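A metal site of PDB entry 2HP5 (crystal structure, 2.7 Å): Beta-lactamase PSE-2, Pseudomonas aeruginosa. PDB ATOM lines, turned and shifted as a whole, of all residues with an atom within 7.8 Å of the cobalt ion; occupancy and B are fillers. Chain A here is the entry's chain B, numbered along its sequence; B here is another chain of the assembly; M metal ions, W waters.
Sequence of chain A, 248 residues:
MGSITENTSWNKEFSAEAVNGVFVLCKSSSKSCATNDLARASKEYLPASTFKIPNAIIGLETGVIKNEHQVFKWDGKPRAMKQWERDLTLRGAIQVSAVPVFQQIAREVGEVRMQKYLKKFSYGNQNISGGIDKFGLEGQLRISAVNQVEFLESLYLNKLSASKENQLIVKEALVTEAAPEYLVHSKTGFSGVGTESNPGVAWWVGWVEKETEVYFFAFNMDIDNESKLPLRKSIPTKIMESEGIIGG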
ATOM      1  N   TYR A 156     -11.671   5.939   9.001  1.00  0.00           N
ATOM      2  CA  TYR A 156     -12.627   5.667  10.076  1.00  0.00           C
ATOM      3  C   TYR A 156     -13.462   4.418   9.761  1.00  0.00           C
ATOM      4  O   TYR A 156     -13.606   3.518  10.589  1.00  0.00           O
ATOM      5  CB  TYR A 156     -13.498   6.887  10.384  1.00  0.00           C
ATOM      6  CG  TYR A 156     -14.740   6.559  11.198  1.00  0.00           C
ATOM      7  CD1 TYR A 156     -14.636   6.133  12.512  1.00  0.00           C
ATOM      8  CD2 TYR A 156     -16.008   6.669  10.632  1.00  0.00           C
ATOM      9  CE1 TYR A 156     -15.783   5.822  13.243  1.00  0.00           C
ATOM     10  CE2 TYR A 156     -17.159   6.364  11.356  1.00  0.00           C
ATOM     11  CZ  TYR A 156     -17.028   5.943  12.663  1.00  0.00           C
ATOM     12  OH  TYR A 156     -18.159   5.618  13.389  1.00  0.00           O
ATOM     13  N   LEU A 168      -6.686   0.781  12.855  1.00  0.00           N
ATOM     14  CA  LEU A 168      -7.058   0.931  14.252  1.00  0.00           C
ATOM     15  C   LEU A 168      -5.909   1.497  15.098  1.00  0.00           C
ATOM     16  O   LEU A 168      -6.125   2.388  15.925  1.00  0.00           O
ATOM     17  CB  LEU A 168      -7.527  -0.405  14.825  1.00  0.00           C
ATOM     18  CG  LEU A 168      -8.869  -0.988  14.406  1.00  0.00           C
ATOM     19  CD1 LEU A 168      -8.915  -2.430  14.814  1.00  0.00           C
ATOM     20  CD2 LEU A 168     -10.051  -0.229  15.020  1.00  0.00           C
ATOM     21  N   LYS A 171      -5.465   5.203  14.404  1.00  0.00           N
ATOM     22  CA  LYS A 171      -6.596   5.936  14.961  1.00  0.00           C
ATOM     23  C   LYS A 171      -6.436   6.279  16.445  1.00  0.00           C
ATOM     24  O   LYS A 171      -6.659   7.418  16.850  1.00  0.00           O
ATOM     25  CB  LYS A 171      -7.880   5.177  14.700  1.00  0.00           C
ATOM     26  CG  LYS A 171      -8.792   5.837  13.676  1.00  0.00           C
ATOM     27  CD  LYS A 171      -9.272   4.897  12.541  1.00  0.00           C
ATOM     28  CE  LYS A 171      -9.789   3.550  13.004  1.00  0.00           C
ATOM     29  NZ  LYS A 171     -10.740   2.979  12.024  1.00  0.00           N
ATOM     30  N   GLU A 172      -6.030   5.308  17.258  1.00  0.00           N
ATOM     31  CA  GLU A 172      -5.742   5.560  18.665  1.00  0.00           C
ATOM     32  C   GLU A 172      -4.640   6.604  18.790  1.00  0.00           C
ATOM     33  O   GLU A 172      -4.722   7.509  19.625  1.00  0.00           O
ATOM     34  CB  GLU A 172      -5.377   4.267  19.411  1.00  0.00           C
ATOM     35  CG  GLU A 172      -4.641   4.459  20.734  1.00  0.00           C
ATOM     36  CD  GLU A 172      -5.078   3.480  21.806  1.00  0.00           C
ATOM     37  OE1 GLU A 172      -4.237   3.091  22.646  1.00  0.00           O
ATOM     38  OE2 GLU A 172      -6.271   3.107  21.836  1.00  0.00           O
ATOM     39  N   VAL A 175      -5.901  10.062  18.661  1.00  0.00           N
ATOM     40  CA  VAL A 175      -6.759  10.524  19.750  1.00  0.00           C
ATOM     41  C   VAL A 175      -6.112  11.731  20.401  1.00  0.00           C
ATOM     42  O   VAL A 175      -5.010  11.632  20.940  1.00  0.00           O
ATOM     43  CB  VAL A 175      -6.983   9.440  20.832  1.00  0.00           C
ATOM     44  CG1 VAL A 175      -7.753  10.011  22.012  1.00  0.00           C
ATOM     45  CG2 VAL A 175      -7.721   8.260  20.257  1.00  0.00           C
ATOM     46  N   LEU A 183     -15.238  11.743  21.578  1.00  0.00           N
ATOM     47  CA  LEU A 183     -13.856  11.377  21.336  1.00  0.00           C
ATOM     48  C   LEU A 183     -13.365  12.077  20.080  1.00  0.00           C
ATOM     49  O   LEU A 183     -13.969  11.987  19.014  1.00  0.00           O
ATOM     50  CB  LEU A 183     -13.720   9.849  21.210  1.00  0.00           C
ATOM     51  CG  LEU A 183     -12.343   9.190  21.276  1.00  0.00           C
ATOM     52  CD1 LEU A 183     -11.801   9.167  22.700  1.00  0.00           C
ATOM     53  CD2 LEU A 183     -12.461   7.775  20.754  1.00  0.00           C
ATOM     54  N   VAL A 184     -12.253  12.802  20.224  1.00  0.00           N
ATOM     55  CA  VAL A 184     -11.695  13.609  19.150  1.00  0.00           C
ATOM     56  C   VAL A 184     -10.415  12.949  18.629  1.00  0.00           C
ATOM     57  O   VAL A 184      -9.469  12.726  19.381  1.00  0.00           O
ATOM     58  CB  VAL A 184     -11.389  15.067  19.625  1.00  0.00           C
ATOM     59  CG1 VAL A 184     -10.997  15.939  18.458  1.00  0.00           C
ATOM     60  CG2 VAL A 184     -12.589  15.666  20.320  1.00  0.00           C
ATOM     61  N   HIS A 185     -10.421  12.642  17.338  1.00  0.00           N
ATOM     62  CA  HIS A 185      -9.235  12.208  16.621  1.00  0.00           C
ATOM     63  C   HIS A 185      -8.825  13.395  15.773  1.00  0.00           C
ATOM     64  O   HIS A 185      -9.634  13.881  14.971  1.00  0.00           O
ATOM     65  CB  HIS A 185      -9.534  11.021  15.709  1.00  0.00           C
ATOM     66  CG  HIS A 185      -9.889   9.756  16.441  1.00  0.00           C
ATOM     67  ND1 HIS A 185      -8.989   8.730  16.621  1.00  0.00           N
ATOM     68  CD2 HIS A 185     -11.047   9.346  17.013  1.00  0.00           C
ATOM     69  CE1 HIS A 185      -9.577   7.746  17.276  1.00  0.00           C
ATOM     70  NE2 HIS A 185     -10.818   8.092  17.522  1.00  0.00           N
ATOM     71  N   TRP A 207     -11.863  14.103  13.144  1.00  0.00           N
ATOM     72  CA  TRP A 207     -13.292  13.872  13.341  1.00  0.00           C
ATOM     73  C   TRP A 207     -13.689  13.855  14.816  1.00  0.00           C
ATOM     74  O   TRP A 207     -12.874  13.511  15.678  1.00  0.00           O
ATOM     75  CB  TRP A 207     -13.761  12.596  12.622  1.00  0.00           C
ATOM     76  CG  TRP A 207     -13.185  11.306  13.113  1.00  0.00           C
ATOM     77  CD1 TRP A 207     -13.764  10.448  14.005  1.00  0.00           C
ATOM     78  CD2 TRP A 207     -11.938  10.709  12.727  1.00  0.00           C
ATOM     79  NE1 TRP A 207     -12.950   9.356  14.197  1.00  0.00           N
ATOM     80  CE2 TRP A 207     -11.832   9.493  13.431  1.00  0.00           C
ATOM     81  CE3 TRP A 207     -10.908  11.088  11.857  1.00  0.00           C
ATOM     82  CZ2 TRP A 207     -10.727   8.647  13.287  1.00  0.00           C
ATOM     83  CZ3 TRP A 207      -9.814  10.252  11.711  1.00  0.00           C
ATOM     84  CH2 TRP A 207      -9.729   9.048  12.435  1.00  0.00           C
ATOM     85  N   VAL A 208     -14.934  14.251  15.091  1.00  0.00           N
ATOM     86  CA  VAL A 208     -15.495  14.266  16.447  1.00  0.00           C
ATOM     87  C   VAL A 208     -16.628  13.249  16.578  1.00  0.00           C
ATOM     88  O   VAL A 208     -17.672  13.398  15.958  1.00  0.00           O
ATOM     89  CB  VAL A 208     -16.055  15.688  16.838  1.00  0.00           C
ATOM     90  CG1 VAL A 208     -16.630  15.684  18.239  1.00  0.00           C
ATOM     91  CG2 VAL A 208     -14.976  16.745  16.736  1.00  0.00           C
ATOM     92  N   GLU A 209     -16.404  12.213  17.378  1.00  0.00           N
ATOM     93  CA  GLU A 209     -17.470  11.241  17.666  1.00  0.00           C
ATOM     94  C   GLU A 209     -18.263  11.721  18.878  1.00  0.00           C
ATOM     95  O   GLU A 209     -17.750  11.765  19.987  1.00  0.00           O
ATOM     96  CB  GLU A 209     -16.907   9.845  17.952  1.00  0.00           C
ATOM     97  CG  GLU A 209     -15.758   9.435  17.051  1.00  0.00           C
ATOM     98  CD  GLU A 209     -15.642   7.934  16.902  1.00  0.00           C
ATOM     99  OE1 GLU A 209     -16.641   7.298  16.520  1.00  0.00           O
ATOM    100  OE2 GLU A 209     -14.548   7.394  17.164  1.00  0.00           O
ATOM    101  N   GLU B  68     -16.946  -2.008  15.817  1.00  0.00           N
ATOM    102  CA  GLU B  68     -16.905  -0.788  16.651  1.00  0.00           C
ATOM    103  C   GLU B  68     -17.990   0.250  16.343  1.00  0.00           C
ATOM    104  O   GLU B  68     -18.342   1.037  17.215  1.00  0.00           O
ATOM    105  CB  GLU B  68     -15.520  -0.129  16.635  1.00  0.00           C
ATOM    106  CG  GLU B  68     -15.111   0.543  15.323  1.00  0.00           C
ATOM    107  CD  GLU B  68     -14.437  -0.413  14.362  1.00  0.00           C
ATOM    108  OE1 GLU B  68     -14.886  -1.563  14.244  1.00  0.00           O
ATOM    109  OE2 GLU B  68     -13.448   0.000  13.716  1.00  0.00           O
ATOM    110  N   HIS B  69     -18.518   0.238  15.117  1.00  0.00           N
ATOM    111  CA  HIS B  69     -19.558   1.200  14.713  1.00  0.00           C
ATOM    112  C   HIS B  69     -20.950   0.626  14.926  1.00  0.00           C
ATOM    113  O   HIS B  69     -21.904   1.041  14.252  1.00  0.00           O
ATOM    114  CB  HIS B  69     -19.406   1.646  13.248  1.00  0.00           C
ATOM    115  CG  HIS B  69     -17.990   1.910  12.823  1.00  0.00           C
ATOM    116  ND1 HIS B  69     -17.408   1.291  11.742  1.00  0.00           N
ATOM    117  CD2 HIS B  69     -17.040   2.723  13.345  1.00  0.00           C
ATOM    118  CE1 HIS B  69     -16.161   1.709  11.615  1.00  0.00           C
ATOM    119  NE2 HIS B  69     -15.911   2.579  12.576  1.00  0.00           N
ATOM    120  N   ARG B  91     -18.080   2.701  23.024  1.00  0.00           N
ATOM    121  CA  ARG B  91     -17.501   3.624  24.005  1.00  0.00           C
ATOM    122  C   ARG B  91     -18.593   4.212  24.904  1.00  0.00           C
ATOM    123  O   ARG B  91     -18.449   4.229  26.127  1.00  0.00           O
ATOM    124  CB  ARG B  91     -16.680   4.740  23.328  1.00  0.00           C
ATOM    125  CG  ARG B  91     -15.938   5.639  24.340  1.00  0.00           C
ATOM    126  CD  ARG B  91     -15.188   6.822  23.736  1.00  0.00           C
ATOM    127  NE  ARG B  91     -14.326   7.401  24.760  1.00  0.00           N
ATOM    128  CZ  ARG B  91     -14.603   8.498  25.471  1.00  0.00           C
ATOM    129  NH1 ARG B  91     -13.752   8.924  26.402  1.00  0.00           N
ATOM    130  NH2 ARG B  91     -15.722   9.181  25.269  1.00  0.00           N
ATOM    131  N   GLU B 172      -9.651   1.263  22.501  1.00  0.00           N
ATOM    132  CA  GLU B 172     -10.092   2.623  22.159  1.00  0.00           C
ATOM    133  C   GLU B 172     -11.355   3.025  22.925  1.00  0.00           C
ATOM    134  O   GLU B 172     -11.469   4.161  23.403  1.00  0.00           O
ATOM    135  CB  GLU B 172     -10.269   2.783  20.645  1.00  0.00           C
ATOM    136  CG  GLU B 172     -11.405   3.716  20.218  1.00  0.00           C
ATOM    137  CD  GLU B 172     -11.027   4.659  19.088  1.00  0.00           C
ATOM    138  OE1 GLU B 172      -9.847   4.674  18.660  1.00  0.00           O
ATOM    139  OE2 GLU B 172     -11.925   5.406  18.636  1.00  0.00           O
ATOM    140  N   ALA B 173     -12.311   2.093  23.034  1.00  0.00           N
ATOM    141  CA  ALA B 173     -13.511   2.309  23.825  1.00  0.00           C
ATOM    142  C   ALA B 173     -13.194   2.766  25.264  1.00  0.00           C
ATOM    143  O   ALA B 173     -14.023   3.421  25.910  1.00  0.00           O
ATOM    144  CB  ALA B 173     -14.375   1.057  23.835  1.00  0.00           C
HETATM  145 CO    CO M   1     -12.458   6.777  17.304  1.00  0.00          CO
HETATM  146  O   HOH W   1     -12.419   5.590  15.380  1.00  0.00           O
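The backbone carbonyl oxygen (O) of His 185 sits at hydrogen-bond distance from the backbone NH (N) of Trp 207 (2.9 Å).
ND1 of His 185 is in hydrogen-bond range of O of Lys 171 (2.7 Å).
N of Glu 209 sits at hydrogen-bond distance from O of Leu 183 (2.9 Å).
CD2 of Leu 183 touches the cobalt ion (3.6 Å).
The cobalt ion is bound by OE2 of Glu 172 of chain B, NE2 of His 185, OE2 of Glu 209 and water W1.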
